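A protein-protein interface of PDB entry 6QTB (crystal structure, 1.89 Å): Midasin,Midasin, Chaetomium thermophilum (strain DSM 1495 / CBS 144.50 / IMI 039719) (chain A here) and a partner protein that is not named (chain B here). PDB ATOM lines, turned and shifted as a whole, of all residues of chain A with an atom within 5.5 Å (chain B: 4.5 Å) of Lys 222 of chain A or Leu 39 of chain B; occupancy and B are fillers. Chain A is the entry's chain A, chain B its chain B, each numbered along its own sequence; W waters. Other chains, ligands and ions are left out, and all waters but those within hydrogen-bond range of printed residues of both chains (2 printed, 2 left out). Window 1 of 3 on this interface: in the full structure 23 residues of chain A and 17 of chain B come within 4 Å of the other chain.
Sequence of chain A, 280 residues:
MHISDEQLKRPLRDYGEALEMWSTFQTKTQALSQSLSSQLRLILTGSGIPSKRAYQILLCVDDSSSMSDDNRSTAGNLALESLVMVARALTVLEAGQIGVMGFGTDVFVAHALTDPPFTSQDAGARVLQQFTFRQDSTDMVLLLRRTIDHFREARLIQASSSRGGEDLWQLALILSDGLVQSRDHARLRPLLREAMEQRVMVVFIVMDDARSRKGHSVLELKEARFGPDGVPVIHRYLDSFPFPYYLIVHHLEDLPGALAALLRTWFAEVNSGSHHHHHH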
ATOM      1  N   VAL A 180      13.030 -13.045  -2.893  1.00  0.00           N
ATOM      2  CA  VAL A 180      12.951 -13.222  -1.463  1.00  0.00           C
ATOM      3  C   VAL A 180      11.646 -12.586  -1.038  1.00  0.00           C
ATOM      4  O   VAL A 180      11.079 -11.743  -1.747  1.00  0.00           O
ATOM      5  CB  VAL A 180      14.152 -12.644  -0.691  1.00  0.00           C
ATOM      6  CG1 VAL A 180      15.499 -13.247  -1.264  1.00  0.00           C
ATOM      7  CG2 VAL A 180      14.215 -11.146  -0.757  1.00  0.00           C
ATOM      8  N   SER A 182       9.230 -10.066   0.471  1.00  0.00           N
ATOM      9  CA  SER A 182       9.408  -8.615   0.427  1.00  0.00           C
ATOM     10  C   SER A 182       9.755  -8.061   1.784  1.00  0.00           C
ATOM     11  O   SER A 182      10.497  -7.072   1.893  1.00  0.00           O
ATOM     12  CB  SER A 182       8.134  -7.947  -0.085  1.00  0.00           C
ATOM     13  OG  SER A 182       8.113  -8.111  -1.483  1.00  0.00           O
ATOM     14  N   LEU A 219      12.350  -7.999 -14.061  1.00  0.00           N
ATOM     15  CA  LEU A 219      12.192  -6.559 -14.186  1.00  0.00           C
ATOM     16  C   LEU A 219      10.717  -6.167 -14.222  1.00  0.00           C
ATOM     17  O   LEU A 219      10.374  -5.013 -13.937  1.00  0.00           O
ATOM     18  CB  LEU A 219      12.861  -6.004 -15.460  1.00  0.00           C
ATOM     19  CG  LEU A 219      14.372  -6.226 -15.521  1.00  0.00           C
ATOM     20  CD1 LEU A 219      14.868  -5.741 -16.881  1.00  0.00           C
ATOM     21  CD2 LEU A 219      15.027  -5.531 -14.365  1.00  0.00           C
ATOM     22  N   GLU A 220       9.855  -7.074 -14.655  1.00  0.00           N
ATOM     23  CA  GLU A 220       8.418  -6.769 -14.711  1.00  0.00           C
ATOM     24  C   GLU A 220       7.621  -7.446 -13.614  1.00  0.00           C
ATOM     25  O   GLU A 220       6.368  -7.379 -13.635  1.00  0.00           O
ATOM     26  CB  GLU A 220       7.832  -7.202 -16.059  1.00  0.00           C
ATOM     27  CG  GLU A 220       8.702  -6.956 -17.263  1.00  0.00           C
ATOM     28  CD  GLU A 220       8.362  -5.657 -17.928  1.00  0.00           C
ATOM     29  OE1 GLU A 220       8.030  -4.687 -17.198  1.00  0.00           O
ATOM     30  OE2 GLU A 220       8.384  -5.620 -19.182  1.00  0.00           O
ATOM     31  N   LEU A 221       8.295  -8.058 -12.642  1.00  0.00           N
ATOM     32  CA  LEU A 221       7.584  -8.656 -11.525  1.00  0.00           C
ATOM     33  C   LEU A 221       6.996  -7.565 -10.642  1.00  0.00           C
ATOM     34  O   LEU A 221       7.694  -6.651 -10.185  1.00  0.00           O
ATOM     35  CB  LEU A 221       8.509  -9.569 -10.696  1.00  0.00           C
ATOM     36  CG  LEU A 221       7.879 -10.214  -9.470  1.00  0.00           C
ATOM     37  CD1 LEU A 221       6.704 -11.146  -9.893  1.00  0.00           C
ATOM     38  CD2 LEU A 221       8.937 -11.029  -8.631  1.00  0.00           C
ATOM     39  N   LYS A 222       5.703  -7.661 -10.375  1.00  0.00           N
ATOM     40  CA  LYS A 222       5.024  -6.694  -9.537  1.00  0.00           C
ATOM     41  C   LYS A 222       4.634  -7.373  -8.239  1.00  0.00           C
ATOM     42  O   LYS A 222       4.688  -8.604  -8.126  1.00  0.00           O
ATOM     43  CB  LYS A 222       3.732  -6.163 -10.217  1.00  0.00           C
ATOM     44  CG  LYS A 222       3.931  -5.569 -11.615  1.00  0.00           C
ATOM     45  CD  LYS A 222       4.525  -4.220 -11.598  1.00  0.00           C
ATOM     46  CE  LYS A 222       4.437  -3.560 -13.026  1.00  0.00           C
ATOM     47  NZ  LYS A 222       5.303  -4.250 -14.034  1.00  0.00           N
ATOM     48  N   GLU A 223       4.158  -6.575  -7.277  1.00  0.00           N
ATOM     49  CA  GLU A 223       3.611  -7.153  -6.058  1.00  0.00           C
ATOM     50  C   GLU A 223       2.375  -6.391  -5.603  1.00  0.00           C
ATOM     51  O   GLU A 223       2.355  -5.159  -5.635  1.00  0.00           O
ATOM     52  CB  GLU A 223       4.600  -7.157  -4.903  1.00  0.00           C
ATOM     53  CG  GLU A 223       5.270  -5.912  -4.600  1.00  0.00           C
ATOM     54  CD  GLU A 223       6.145  -6.105  -3.366  1.00  0.00           C
ATOM     55  OE1 GLU A 223       5.606  -6.481  -2.289  1.00  0.00           O
ATOM     56  OE2 GLU A 223       7.375  -5.988  -3.497  1.00  0.00           O
ATOM     57  N   ALA A 224       1.365  -7.138  -5.156  1.00  0.00           N
ATOM     58  CA  ALA A 224       0.088  -6.585  -4.702  1.00  0.00           C
ATOM     59  C   ALA A 224       0.039  -6.560  -3.177  1.00  0.00           C
ATOM     60  O   ALA A 224       0.306  -7.577  -2.523  1.00  0.00           O
ATOM     61  CB  ALA A 224      -1.095  -7.396  -5.241  1.00  0.00           C
ATOM     62  N   ILE A 234      -0.349  -1.867  -6.249  1.00  0.00           N
ATOM     63  CA  ILE A 234       0.633  -2.689  -6.946  1.00  0.00           C
ATOM     64  C   ILE A 234       1.889  -1.868  -7.198  1.00  0.00           C
ATOM     65  O   ILE A 234       1.809  -0.747  -7.702  1.00  0.00           O
ATOM     66  CB  ILE A 234       0.019  -3.241  -8.231  1.00  0.00           C
ATOM     67  CG1 ILE A 234      -1.163  -4.144  -7.814  1.00  0.00           C
ATOM     68  CG2 ILE A 234       1.054  -4.007  -9.045  1.00  0.00           C
ATOM     69  CD1 ILE A 234      -1.939  -4.644  -8.971  1.00  0.00           C
ATOM     70  N   HIS A 235       3.046  -2.447  -6.867  1.00  0.00           N
ATOM     71  CA  HIS A 235       4.364  -1.830  -6.924  1.00  0.00           C
ATOM     72  C   HIS A 235       5.272  -2.770  -7.710  1.00  0.00           C
ATOM     73  O   HIS A 235       4.987  -3.961  -7.764  1.00  0.00           O
ATOM     74  CB  HIS A 235       5.012  -1.720  -5.527  1.00  0.00           C
ATOM     75  CG  HIS A 235       4.190  -1.020  -4.500  1.00  0.00           C
ATOM     76  ND1 HIS A 235       4.191   0.350  -4.352  1.00  0.00           N
ATOM     77  CD2 HIS A 235       3.380  -1.502  -3.530  1.00  0.00           C
ATOM     78  CE1 HIS A 235       3.401   0.686  -3.350  1.00  0.00           C
ATOM     79  NE2 HIS A 235       2.891  -0.418  -2.837  1.00  0.00           N
ATOM     80  N   ARG A 236       6.407  -2.267  -8.247  1.00  0.00           N
ATOM     81  CA  ARG A 236       7.397  -3.175  -8.851  1.00  0.00           C
ATOM     82  C   ARG A 236       8.207  -3.841  -7.738  1.00  0.00           C
ATOM     83  O   ARG A 236       8.637  -3.170  -6.792  1.00  0.00           O
ATOM     84  CB  ARG A 236       8.330  -2.403  -9.803  1.00  0.00           C
ATOM     85  CG  ARG A 236       7.498  -1.654 -10.845  1.00  0.00           C
ATOM     86  CD  ARG A 236       8.315  -0.812 -11.833  1.00  0.00           C
ATOM     87  NE  ARG A 236       9.187   0.131 -11.146  1.00  0.00           N
ATOM     88  CZ  ARG A 236       9.823   1.101 -11.772  1.00  0.00           C
ATOM     89  NH1 ARG A 236      10.631   1.930 -11.107  1.00  0.00           N
ATOM     90  NH2 ARG A 236       9.663   1.207 -13.072  1.00  0.00           N
ATOM     91  N   TYR A 237       8.374  -5.173  -7.824  1.00  0.00           N
ATOM     92  CA  TYR A 237       9.091  -5.897  -6.774  1.00  0.00           C
ATOM     93  C   TYR A 237      10.481  -5.311  -6.535  1.00  0.00           C
ATOM     94  O   TYR A 237      10.887  -5.121  -5.385  1.00  0.00           O
ATOM     95  CB  TYR A 237       9.202  -7.387  -7.164  1.00  0.00           C
ATOM     96  CG  TYR A 237      10.166  -8.160  -6.347  1.00  0.00           C
ATOM     97  CD1 TYR A 237       9.850  -8.537  -5.064  1.00  0.00           C
ATOM     98  CD2 TYR A 237      11.429  -8.482  -6.858  1.00  0.00           C
ATOM     99  CE1 TYR A 237      10.794  -9.284  -4.263  1.00  0.00           C
ATOM    100  CE2 TYR A 237      12.355  -9.188  -6.100  1.00  0.00           C
ATOM    101  CZ  TYR A 237      12.014  -9.598  -4.810  1.00  0.00           C
ATOM    102  OH  TYR A 237      12.893 -10.278  -4.005  1.00  0.00           O
ATOM    103  N   GLN B  17       4.290 -14.190   0.950  1.00  0.00           N
ATOM    104  CA  GLN B  17       3.863 -13.948  -0.418  1.00  0.00           C
ATOM    105  C   GLN B  17       4.067 -15.189  -1.269  1.00  0.00           C
ATOM    106  O   GLN B  17       4.994 -15.962  -1.057  1.00  0.00           O
ATOM    107  CB  GLN B  17       4.632 -12.819  -1.054  1.00  0.00           C
ATOM    108  CG  GLN B  17       4.446 -11.463  -0.415  1.00  0.00           C
ATOM    109  CD  GLN B  17       5.568 -10.551  -0.881  1.00  0.00           C
ATOM    110  OE1 GLN B  17       6.781 -10.874  -0.724  1.00  0.00           O
ATOM    111  NE2 GLN B  17       5.195  -9.456  -1.505  1.00  0.00           N
ATOM    112  N   VAL B  18       3.206 -15.340  -2.249  1.00  0.00           N
ATOM    113  CA  VAL B  18       3.276 -16.388  -3.263  1.00  0.00           C
ATOM    114  C   VAL B  18       3.427 -15.754  -4.635  1.00  0.00           C
ATOM    115  O   VAL B  18       2.739 -14.760  -4.920  1.00  0.00           O
ATOM    116  CB  VAL B  18       1.980 -17.230  -3.214  1.00  0.00           C
ATOM    117  CG1 VAL B  18       1.921 -18.235  -4.387  1.00  0.00           C
ATOM    118  CG2 VAL B  18       1.976 -17.950  -1.905  1.00  0.00           C
ATOM    119  N   LYS B  19       4.280 -16.333  -5.508  1.00  0.00           N
ATOM    120  CA  LYS B  19       4.406 -15.793  -6.866  1.00  0.00           C
ATOM    121  C   LYS B  19       3.393 -16.434  -7.816  1.00  0.00           C
ATOM    122  O   LYS B  19       3.322 -17.666  -7.935  1.00  0.00           O
ATOM    123  CB  LYS B  19       5.831 -15.988  -7.397  1.00  0.00           C
ATOM    124  CG  LYS B  19       5.988 -15.326  -8.747  1.00  0.00           C
ATOM    125  CD  LYS B  19       7.496 -15.303  -9.216  1.00  0.00           C
ATOM    126  CE  LYS B  19       7.477 -15.282 -10.748  1.00  0.00           C
ATOM    127  NZ  LYS B  19       8.747 -15.700 -11.375  1.00  0.00           N
ATOM    128  N   SER B  34       3.546  -7.219 -19.151  1.00  0.00           N
ATOM    129  CA  SER B  34       4.190  -6.597 -18.002  1.00  0.00           C
ATOM    130  C   SER B  34       3.372  -6.673 -16.721  1.00  0.00           C
ATOM    131  O   SER B  34       3.913  -6.360 -15.648  1.00  0.00           O
ATOM    132  CB  SER B  34       4.499  -5.135 -18.353  1.00  0.00           C
ATOM    133  OG  SER B  34       3.300  -4.351 -18.381  1.00  0.00           O
ATOM    134  N   GLN B  37       2.792 -11.127 -14.046  1.00  0.00           N
ATOM    135  CA  GLN B  37       3.526 -11.779 -12.954  1.00  0.00           C
ATOM    136  C   GLN B  37       3.395 -10.960 -11.696  1.00  0.00           C
ATOM    137  O   GLN B  37       3.822  -9.795 -11.688  1.00  0.00           O
ATOM    138  CB  GLN B  37       5.015 -11.900 -13.268  1.00  0.00           C
ATOM    139  CG  GLN B  37       5.478 -12.505 -14.493  1.00  0.00           C
ATOM    140  CD  GLN B  37       6.977 -12.160 -14.577  1.00  0.00           C
ATOM    141  OE1 GLN B  37       7.339 -11.112 -15.126  1.00  0.00           O
ATOM    142  NE2 GLN B  37       7.820 -12.940 -13.871  1.00  0.00           N
ATOM    143  N   LEU B  38       2.883 -11.580 -10.602  1.00  0.00           N
ATOM    144  CA  LEU B  38       2.546 -10.815  -9.409  1.00  0.00           C
ATOM    145  C   LEU B  38       2.866 -11.612  -8.135  1.00  0.00           C
ATOM    146  O   LEU B  38       2.490 -12.785  -8.004  1.00  0.00           O
ATOM    147  CB  LEU B  38       1.018 -10.447  -9.435  1.00  0.00           C
ATOM    148  CG  LEU B  38       0.416  -9.356  -8.538  1.00  0.00           C
ATOM    149  CD1 LEU B  38       0.997  -7.956  -8.856  1.00  0.00           C
ATOM    150  CD2 LEU B  38      -1.156  -9.251  -8.691  1.00  0.00           C
ATOM    151  N   LEU B  39       3.467 -10.950  -7.154  1.00  0.00           N
ATOM    152  CA  LEU B  39       3.513 -11.510  -5.793  1.00  0.00           C
ATOM    153  C   LEU B  39       2.249 -11.107  -5.060  1.00  0.00           C
ATOM    154  O   LEU B  39       1.892  -9.919  -5.065  1.00  0.00           O
ATOM    155  CB  LEU B  39       4.714 -10.982  -5.007  1.00  0.00           C
ATOM    156  CG  LEU B  39       6.079 -11.365  -5.558  1.00  0.00           C
ATOM    157  CD1 LEU B  39       7.114 -10.716  -4.586  1.00  0.00           C
ATOM    158  CD2 LEU B  39       6.241 -12.874  -5.673  1.00  0.00           C
ATOM    159  N   VAL B  40       1.580 -12.081  -4.446  1.00  0.00           N
ATOM    160  CA  VAL B  40       0.328 -11.831  -3.729  1.00  0.00           C
ATOM    161  C   VAL B  40       0.429 -12.425  -2.330  1.00  0.00           C
ATOM    162  O   VAL B  40       1.191 -13.382  -2.098  1.00  0.00           O
ATOM    163  CB  VAL B  40      -0.889 -12.396  -4.508  1.00  0.00           C
ATOM    164  CG1 VAL B  40      -0.935 -11.695  -5.937  1.00  0.00           C
ATOM    165  CG2 VAL B  40      -0.832 -13.894  -4.645  1.00  0.00           C
HETATM  166  O   HOH W   1       6.874 -10.707   2.720  1.00  0.00           O
HETATM  167  O   HOH W   2       2.672  -9.058  -1.850  1.00  0.00           O
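OE1 of Gln 17 of chain B lies within hydrogen-bond range of N of Ser 182 of chain A, 2.8 Å away. The side-chain amino group (NZ) of Lys 222 of chain A is in hydrogen-bond range of the backbone carbonyl oxygen (O) of Ser 34 of chain B (3.0 Å). N of Lys 222 of chain A is in hydrogen-bond range of O of Gln 37 of chain B, at 3.1 Å. The backbone carbonyl oxygen of Lys 222 of chain A lies within hydrogen-bond range of the backbone NH of Leu 39 of chain B, at 2.8 Å. The side-chain carboxylate (OE1) of Glu 223 of chain A is in hydrogen-bond range of the side-chain amide nitrogen (NE2) of Gln 17 of chain B. The backbone NH of Ala 224 of chain A lies within hydrogen-bond range of the backbone carbonyl oxygen of Leu 39 of chain B (2.8 Å). O of Glu 220 of chain A lies close to O of Ser 34 of chain B.
The backbone NH (N) of Val 180 of chain A sits at hydrogen-bond distance from the side-chain hydroxyl (OH) of Tyr 237 of chain A. The side-chain hydroxyl (OG) of Ser 182 of chain A lies within hydrogen-bond range of the side-chain carboxylate (OE2) of Glu 223 of chain A. The backbone carbonyl oxygen of Glu 220 of chain A sits at hydrogen-bond distance from the side-chain amino group of Lys 222 of chain A (3.3 Å). The backbone carbonyl oxygen (O) of Leu 221 of chain A is in hydrogen-bond range of the backbone NH (N) of Tyr 237 of chain A, at 2.9 Å. The backbone carbonyl oxygen (O) of His 235 of chain A lies within hydrogen-bond range of the backbone NH (N) of Glu 223 of chain A (2.8 Å).
Among the printed residues, pairs that only touch across the chains: Glu 220 of chain A with Gln 37 of chain B, Leu 221 of chain A with Gln 37 of chain B, Leu 221 of chain A with Leu 38 of chain B, Lys 222 of chain A with Leu 38 of chain B, Glu 223 of chain A with Leu 38 of chain B, Glu 223 of chain A with Leu 39 of chain B, Ala 224 of chain A with Leu 38 of chain B, Ile 234 of chain A with Leu 38 of chain B and Tyr 237 of chain A with Leu 39 of chain B.
Lys 222 of chain A touches just these residues of chain B: Ser 34, Gln 37, Leu 38 and Leu 39. Of chain A, only Lys 222 (2.8 Å), Glu 223 (3.4 Å), Ala 224 (2.8 Å) and Tyr 237 (3.5 Å) come within 4 Å of Leu 39 of chain B. Of the printed residues of chain B, Glu 220 of chain A touches Ser 34 and Gln 37. Printed residues of chain A within 4 Å of Ser 34 of chain B: Glu 220 and Lys 222. Printed residues of chain B within 4 Å of Ile 234 of chain A: Leu 38. The nearest printed residue of chain B that does not touch Lys 222 of chain A is Val 40 of chain B (5.9 Å). The nearest residue of chain A that does not touch Leu 39 of chain B is Ser 182 of chain A (4.2 Å).
Of the 8 printed residues of chain B, 5 touch a printed residue of chain A. Printed residues of chain A that touch a printed residue of chain B: Ser 182, Glu 220, Leu 221, Lys 222, Glu 223, Ala 224, Ile 234 and Tyr 237. Hydrophobic or aromatic side chains of chain A that line the printed part of chain B: Leu 221, Ala 224, Ile 234 and Tyr 237. Among the printed residues, 16 pairs touch across the chains.
Water W2 lies within hydrogen-bond range of NE2 of Gln 17 of chain B, O of Ala 224 of chain A and O of Leu 39 of chain B. Water W1 lies within hydrogen-bond range of the backbone NH of Ser 182 of chain A and the side-chain amide oxygen of Gln 17 of chain B.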
